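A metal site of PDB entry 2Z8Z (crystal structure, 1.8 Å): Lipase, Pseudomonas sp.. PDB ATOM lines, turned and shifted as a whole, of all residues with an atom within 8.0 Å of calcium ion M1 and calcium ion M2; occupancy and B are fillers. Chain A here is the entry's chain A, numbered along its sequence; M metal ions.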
ATOM      1  N   LYS A 501      15.818 -12.872 -19.333  1.00  0.00           N
ATOM      2  CA  LYS A 501      15.221 -14.081 -19.840  1.00  0.00           C
ATOM      3  C   LYS A 501      14.701 -13.905 -21.251  1.00  0.00           C
ATOM      4  O   LYS A 501      13.890 -12.987 -21.535  1.00  0.00           O
ATOM      5  CB  LYS A 501      14.043 -14.493 -18.931  1.00  0.00           C
ATOM      6  CG  LYS A 501      14.349 -14.671 -17.471  1.00  0.00           C
ATOM      7  CD  LYS A 501      13.064 -15.183 -16.752  1.00  0.00           C
ATOM      8  CE  LYS A 501      13.170 -15.206 -15.253  1.00  0.00           C
ATOM      9  NZ  LYS A 501      14.333 -14.411 -14.675  1.00  0.00           N
ATOM     10  N   ALA A 502      15.158 -14.752 -22.168  1.00  0.00           N
ATOM     11  CA  ALA A 502      14.599 -14.804 -23.502  1.00  0.00           C
ATOM     12  C   ALA A 502      13.196 -15.402 -23.533  1.00  0.00           C
ATOM     13  O   ALA A 502      12.869 -16.261 -22.717  1.00  0.00           O
ATOM     14  CB  ALA A 502      15.452 -15.643 -24.422  1.00  0.00           C
ATOM     15  N   HIS A 503      12.438 -14.989 -24.534  1.00  0.00           N
ATOM     16  CA  HIS A 503      11.117 -15.545 -24.804  1.00  0.00           C
ATOM     17  C   HIS A 503      11.352 -16.714 -25.724  1.00  0.00           C
ATOM     18  O   HIS A 503      12.388 -16.744 -26.372  1.00  0.00           O
ATOM     19  CB  HIS A 503      10.240 -14.478 -25.467  1.00  0.00           C
ATOM     20  CG  HIS A 503      10.015 -13.277 -24.615  1.00  0.00           C
ATOM     21  ND1 HIS A 503      10.708 -12.098 -24.760  1.00  0.00           N
ATOM     22  CD2 HIS A 503       9.171 -13.084 -23.557  1.00  0.00           C
ATOM     23  CE1 HIS A 503      10.325 -11.240 -23.833  1.00  0.00           C
ATOM     24  NE2 HIS A 503       9.373 -11.802 -23.112  1.00  0.00           N
ATOM     25  N   ALA A 504      10.391 -17.644 -25.797  1.00  0.00           N
ATOM     26  CA  ALA A 504      10.519 -18.866 -26.574  1.00  0.00           C
ATOM     27  C   ALA A 504      10.758 -18.633 -28.049  1.00  0.00           C
ATOM     28  O   ALA A 504      11.375 -19.467 -28.697  1.00  0.00           O
ATOM     29  CB  ALA A 504       9.256 -19.795 -26.403  1.00  0.00           C
ATOM     30  N   GLY A 505      10.308 -17.503 -28.601  1.00  0.00           N
ATOM     31  CA  GLY A 505      10.529 -17.195 -30.005  1.00  0.00           C
ATOM     32  C   GLY A 505      12.001 -16.848 -30.390  1.00  0.00           C
ATOM     33  O   GLY A 505      12.402 -16.867 -31.601  1.00  0.00           O
ATOM     34  N   GLY A 506      12.781 -16.582 -29.345  1.00  0.00           N
ATOM     35  CA  GLY A 506      14.193 -16.180 -29.455  1.00  0.00           C
ATOM     36  C   GLY A 506      14.350 -14.670 -29.329  1.00  0.00           C
ATOM     37  O   GLY A 506      13.493 -13.892 -29.777  1.00  0.00           O
ATOM     38  N   ASP A 507      15.441 -14.247 -28.718  1.00  0.00           N
ATOM     39  CA  ASP A 507      15.666 -12.848 -28.472  1.00  0.00           C
ATOM     40  C   ASP A 507      17.160 -12.573 -28.607  1.00  0.00           C
ATOM     41  O   ASP A 507      18.004 -13.486 -28.321  1.00  0.00           O
ATOM     42  CB  ASP A 507      15.281 -12.512 -27.057  1.00  0.00           C
ATOM     43  CG  ASP A 507      13.827 -12.187 -26.908  1.00  0.00           C
ATOM     44  OD1 ASP A 507      13.369 -11.239 -27.577  1.00  0.00           O
ATOM     45  OD2 ASP A 507      13.180 -12.858 -26.078  1.00  0.00           O
ATOM     46  N   LEU A 509      19.758 -10.915 -26.436  1.00  0.00           N
ATOM     47  CA  LEU A 509      19.936 -10.572 -25.051  1.00  0.00           C
ATOM     48  C   LEU A 509      21.170  -9.669 -24.856  1.00  0.00           C
ATOM     49  O   LEU A 509      22.311 -10.084 -25.101  1.00  0.00           O
ATOM     50  CB  LEU A 509      20.099 -11.828 -24.158  1.00  0.00           C
ATOM     51  CG  LEU A 509      18.923 -12.843 -24.238  1.00  0.00           C
ATOM     52  CD1 LEU A 509      19.165 -13.963 -23.382  1.00  0.00           C
ATOM     53  CD2 LEU A 509      17.658 -12.141 -23.861  1.00  0.00           C
ATOM     54  N   ILE A 519      19.581 -15.894 -19.578  1.00  0.00           N
ATOM     55  CA  ILE A 519      18.845 -17.129 -19.627  1.00  0.00           C
ATOM     56  C   ILE A 519      18.138 -17.258 -20.964  1.00  0.00           C
ATOM     57  O   ILE A 519      17.073 -16.722 -21.237  1.00  0.00           O
ATOM     58  CB  ILE A 519      17.840 -17.313 -18.457  1.00  0.00           C
ATOM     59  CG1 ILE A 519      18.443 -16.982 -17.099  1.00  0.00           C
ATOM     60  CG2 ILE A 519      17.305 -18.761 -18.530  1.00  0.00           C
ATOM     61  CD1 ILE A 519      17.423 -16.989 -16.019  1.00  0.00           C
ATOM     62  N   GLY A 520      18.763 -18.003 -21.859  1.00  0.00           N
ATOM     63  CA  GLY A 520      18.167 -18.241 -23.133  1.00  0.00           C
ATOM     64  C   GLY A 520      16.959 -19.139 -23.028  1.00  0.00           C
ATOM     65  O   GLY A 520      16.704 -19.766 -22.000  1.00  0.00           O
ATOM     66  N   GLY A 521      16.227 -19.179 -24.102  1.00  0.00           N
ATOM     67  CA  GLY A 521      15.098 -20.171 -24.229  1.00  0.00           C
ATOM     68  C   GLY A 521      15.274 -21.199 -25.355  1.00  0.00           C
ATOM     69  O   GLY A 521      16.324 -21.341 -25.994  1.00  0.00           O
ATOM     70  N   VAL A 522      14.197 -21.903 -25.640  1.00  0.00           N
ATOM     71  CA  VAL A 522      14.293 -22.974 -26.631  1.00  0.00           C
ATOM     72  C   VAL A 522      14.421 -22.418 -28.008  1.00  0.00           C
ATOM     73  O   VAL A 522      14.665 -23.151 -28.933  1.00  0.00           O
ATOM     74  CB  VAL A 522      13.008 -23.845 -26.603  1.00  0.00           C
ATOM     75  CG1 VAL A 522      12.766 -24.452 -25.234  1.00  0.00           C
ATOM     76  CG2 VAL A 522      11.834 -22.985 -27.028  1.00  0.00           C
ATOM     77  N   GLY A 523      14.226 -21.099 -28.187  1.00  0.00           N
ATOM     78  CA  GLY A 523      14.437 -20.468 -29.467  1.00  0.00           C
ATOM     79  C   GLY A 523      15.902 -20.100 -29.742  1.00  0.00           C
ATOM     80  O   GLY A 523      16.754 -20.321 -28.924  1.00  0.00           O
ATOM     81  N   ASN A 524      16.098 -19.520 -30.918  1.00  0.00           N
ATOM     82  CA  ASN A 524      17.374 -19.089 -31.454  1.00  0.00           C
ATOM     83  C   ASN A 524      17.663 -17.667 -30.919  1.00  0.00           C
ATOM     84  O   ASN A 524      17.119 -16.663 -31.370  1.00  0.00           O
ATOM     85  CB  ASN A 524      17.370 -19.133 -32.969  1.00  0.00           C
ATOM     86  CG  ASN A 524      17.060 -20.510 -33.540  1.00  0.00           C
ATOM     87  OD1 ASN A 524      17.100 -21.518 -32.856  1.00  0.00           O
ATOM     88  ND2 ASN A 524      16.799 -20.535 -34.835  1.00  0.00           N
ATOM     89  N   ASP A 525      18.530 -17.624 -29.939  1.00  0.00           N
ATOM     90  CA  ASP A 525      18.910 -16.446 -29.205  1.00  0.00           C
ATOM     91  C   ASP A 525      20.271 -15.930 -29.710  1.00  0.00           C
ATOM     92  O   ASP A 525      21.110 -16.676 -30.224  1.00  0.00           O
ATOM     93  CB  ASP A 525      18.988 -16.768 -27.729  1.00  0.00           C
ATOM     94  CG  ASP A 525      17.697 -17.378 -27.176  1.00  0.00           C
ATOM     95  OD1 ASP A 525      16.619 -16.775 -27.383  1.00  0.00           O
ATOM     96  OD2 ASP A 525      17.788 -18.504 -26.625  1.00  0.00           O
ATOM     97  N   VAL A 526      20.499 -14.642 -29.519  1.00  0.00           N
ATOM     98  CA  VAL A 526      21.813 -14.039 -29.742  1.00  0.00           C
ATOM     99  C   VAL A 526      22.213 -13.365 -28.418  1.00  0.00           C
ATOM    100  O   VAL A 526      21.561 -12.427 -27.945  1.00  0.00           O
ATOM    101  CB  VAL A 526      21.828 -13.001 -30.882  1.00  0.00           C
ATOM    102  CG1 VAL A 526      23.251 -12.457 -31.035  1.00  0.00           C
ATOM    103  CG2 VAL A 526      21.335 -13.607 -32.186  1.00  0.00           C
ATOM    104  N   PHE A 527      23.255 -13.892 -27.800  1.00  0.00           N
ATOM    105  CA  PHE A 527      23.709 -13.505 -26.486  1.00  0.00           C
ATOM    106  C   PHE A 527      24.854 -12.491 -26.659  1.00  0.00           C
ATOM    107  O   PHE A 527      25.906 -12.810 -27.289  1.00  0.00           O
ATOM    108  CB  PHE A 527      24.278 -14.659 -25.704  1.00  0.00           C
ATOM    109  CG  PHE A 527      23.278 -15.719 -25.342  1.00  0.00           C
ATOM    110  CD1 PHE A 527      22.703 -15.775 -24.067  1.00  0.00           C
ATOM    111  CD2 PHE A 527      22.914 -16.666 -26.279  1.00  0.00           C
ATOM    112  CE1 PHE A 527      21.765 -16.757 -23.735  1.00  0.00           C
ATOM    113  CE2 PHE A 527      21.972 -17.657 -25.957  1.00  0.00           C
ATOM    114  CZ  PHE A 527      21.411 -17.682 -24.674  1.00  0.00           C
ATOM    115  N   GLU A 537      23.291 -18.910 -20.691  1.00  0.00           N
ATOM    116  CA  GLU A 537      22.694 -20.262 -20.807  1.00  0.00           C
ATOM    117  C   GLU A 537      21.860 -20.372 -22.070  1.00  0.00           C
ATOM    118  O   GLU A 537      20.854 -19.652 -22.277  1.00  0.00           O
ATOM    119  CB  GLU A 537      21.839 -20.587 -19.592  1.00  0.00           C
ATOM    120  CG  GLU A 537      22.605 -20.589 -18.279  1.00  0.00           C
ATOM    121  CD  GLU A 537      21.699 -20.396 -17.111  1.00  0.00           C
ATOM    122  OE1 GLU A 537      20.430 -20.576 -17.237  1.00  0.00           O
ATOM    123  OE2 GLU A 537      22.300 -20.077 -16.095  1.00  0.00           O
ATOM    124  N   SER A 538      22.257 -21.310 -22.956  1.00  0.00           N
ATOM    125  CA  SER A 538      21.609 -21.449 -24.251  1.00  0.00           C
ATOM    126  C   SER A 538      20.079 -21.640 -24.160  1.00  0.00           C
ATOM    127  O   SER A 538      19.271 -20.984 -24.881  1.00  0.00           O
ATOM    128  CB  SER A 538      22.153 -22.734 -24.963  1.00  0.00           C
ATOM    129  OG  SER A 538      21.313 -23.062 -26.066  1.00  0.00           O
ATOM    130  N   GLY A 539      19.710 -22.613 -23.359  1.00  0.00           N
ATOM    131  CA  GLY A 539      18.328 -23.043 -23.191  1.00  0.00           C
ATOM    132  C   GLY A 539      17.688 -23.835 -24.342  1.00  0.00           C
ATOM    133  O   GLY A 539      16.502 -24.231 -24.243  1.00  0.00           O
ATOM    134  N   GLY A 540      18.485 -24.124 -25.352  1.00  0.00           N
ATOM    135  CA  GLY A 540      18.106 -24.913 -26.534  1.00  0.00           C
ATOM    136  C   GLY A 540      18.132 -24.069 -27.798  1.00  0.00           C
ATOM    137  O   GLY A 540      18.436 -22.869 -27.775  1.00  0.00           O
ATOM    138  N   GLY A 541      17.846 -24.658 -28.959  1.00  0.00           N
ATOM    139  CA  GLY A 541      17.880 -23.926 -30.202  1.00  0.00           C
ATOM    140  C   GLY A 541      19.295 -23.780 -30.773  1.00  0.00           C
ATOM    141  O   GLY A 541      20.252 -24.414 -30.301  1.00  0.00           O
ATOM    142  N   ALA A 542      19.367 -22.985 -31.816  1.00  0.00           N
ATOM    143  CA  ALA A 542      20.614 -22.671 -32.531  1.00  0.00           C
ATOM    144  C   ALA A 542      20.924 -21.235 -32.140  1.00  0.00           C
ATOM    145  O   ALA A 542      20.377 -20.260 -32.680  1.00  0.00           O
ATOM    146  CB  ALA A 542      20.421 -22.853 -34.040  1.00  0.00           C
ATOM    147  N   ASP A 543      21.847 -21.129 -31.176  1.00  0.00           N
ATOM    148  CA  ASP A 543      22.160 -19.881 -30.529  1.00  0.00           C
ATOM    149  C   ASP A 543      23.517 -19.358 -31.029  1.00  0.00           C
ATOM    150  O   ASP A 543      24.366 -20.099 -31.398  1.00  0.00           O
ATOM    151  CB  ASP A 543      22.212 -20.068 -29.028  1.00  0.00           C
ATOM    152  CG  ASP A 543      20.824 -20.357 -28.400  1.00  0.00           C
ATOM    153  OD1 ASP A 543      19.815 -19.922 -28.967  1.00  0.00           O
ATOM    154  OD2 ASP A 543      20.789 -20.861 -27.264  1.00  0.00           O
ATOM    155  N   THR A 544      23.670 -18.052 -30.937  1.00  0.00           N
ATOM    156  CA  THR A 544      24.879 -17.335 -31.277  1.00  0.00           C
ATOM    157  C   THR A 544      25.352 -16.551 -30.034  1.00  0.00           C
ATOM    158  O   THR A 544      24.540 -15.885 -29.399  1.00  0.00           O
ATOM    159  CB  THR A 544      24.574 -16.314 -32.380  1.00  0.00           C
ATOM    160  OG1 THR A 544      24.056 -16.982 -33.518  1.00  0.00           O
ATOM    161  CG2 THR A 544      25.799 -15.519 -32.751  1.00  0.00           C
ATOM    162  N   PHE A 545      26.645 -16.631 -29.706  1.00  0.00           N
ATOM    163  CA  PHE A 545      27.229 -15.897 -28.562  1.00  0.00           C
ATOM    164  C   PHE A 545      28.290 -14.974 -29.133  1.00  0.00           C
ATOM    165  O   PHE A 545      29.209 -15.436 -29.813  1.00  0.00           O
ATOM    166  CB  PHE A 545      27.864 -16.849 -27.589  1.00  0.00           C
ATOM    167  CG  PHE A 545      26.897 -17.844 -26.997  1.00  0.00           C
ATOM    168  CD1 PHE A 545      26.355 -17.655 -25.752  1.00  0.00           C
ATOM    169  CD2 PHE A 545      26.521 -18.976 -27.712  1.00  0.00           C
ATOM    170  CE1 PHE A 545      25.445 -18.602 -25.193  1.00  0.00           C
ATOM    171  CE2 PHE A 545      25.586 -19.907 -27.176  1.00  0.00           C
ATOM    172  CZ  PHE A 545      25.072 -19.728 -25.915  1.00  0.00           C
ATOM    173  N   GLY A 558      25.387 -24.976 -21.932  1.00  0.00           N
ATOM    174  CA  GLY A 558      24.467 -25.619 -22.901  1.00  0.00           C
ATOM    175  C   GLY A 558      24.857 -25.469 -24.330  1.00  0.00           C
ATOM    176  O   GLY A 558      24.014 -25.596 -25.224  1.00  0.00           O
ATOM    177  N   ASP A 563      25.218 -24.397 -32.294  1.00  0.00           N
ATOM    178  CA  ASP A 563      25.457 -23.075 -31.763  1.00  0.00           C
ATOM    179  C   ASP A 563      26.774 -22.494 -32.293  1.00  0.00           C
ATOM    180  O   ASP A 563      27.600 -23.225 -32.871  1.00  0.00           O
ATOM    181  CB  ASP A 563      25.487 -23.129 -30.265  1.00  0.00           C
ATOM    182  CG  ASP A 563      24.201 -23.731 -29.701  1.00  0.00           C
ATOM    183  OD1 ASP A 563      23.158 -23.398 -30.238  1.00  0.00           O
ATOM    184  OD2 ASP A 563      24.291 -24.559 -28.810  1.00  0.00           O
HETATM  185 CA    CA M   1      18.312 -20.666 -27.078  1.00  0.00          CA
HETATM  186 CA    CA M   2      14.570 -18.519 -26.811  1.00  0.00          CA
HETATM  187 CA    CA M   3      22.143 -25.546 -29.581  1.00  0.00          CA
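The backbone NH (N) of Asp 507 sits close to the side-chain carboxylate (OD1) of Asp 525, at 3.1 Å. O of Asp 525 is in hydrogen-bond range of N of Thr 544. The side-chain hydroxyl (OG) of Ser 538 sits at hydrogen-bond distance from the backbone NH (N) of Gly 540, at 3.1 Å. The backbone NH (N) of Gly 523 lies close to the backbone carbonyl oxygen (O) of Ala 504, at 3.3 Å. The backbone NH of Asp 543 lies close to the side-chain carboxylate of Asp 563. The backbone NH (N) of His 503 lies within hydrogen-bond range of the side-chain carboxylate (OD2) of Asp 507. The backbone NH (N) of Ala 502 sits at hydrogen-bond distance from the backbone carbonyl oxygen (O) of Ile 519.
Six residues have an atom within 4 Å of calcium ion M1: Gly 521, Gly 523, Asp 525, Ser 538, Gly 540 and Asp 543. The nearest printed residue that does not touch calcium ion M1 is Gly 539 (4.2 Å).
Ala 502 touches calcium ion M2 (CB to CA, 3.8 Å). Ala 504 touches calcium ion M2. Gly 506 touches calcium ion M2 (CA to CA, 3.6 Å). N of Val 522 touches calcium ion M2 (3.6 Å). Of the 28 residues printed, 8 come within 4 Å of calcium ion M2. The nearest printed residue that does not touch calcium ion M2 is Asn 524 (4.5 Å).
Calcium ion M1 is bound by OD2 of Asp 525 (2.3 Å), O of Gly 540 (2.3 Å), O of Gly 521 (2.4 Å), O of Ser 538 (2.4 Å), O of Gly 523 (2.4 Å), OD2 of Asp 543 (2.5 Å) and OD1 of Asp 543 (2.5 Å).
Calcium ion M2 is bound by the side-chain carboxylate (OD1) of Asp 525, at 2.8 Å. Calcium ion M2 is bound by O of His 503 (2.8 Å). Slightly farther from calcium ion M2 lies N of Gly 523 (2.9 Å).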
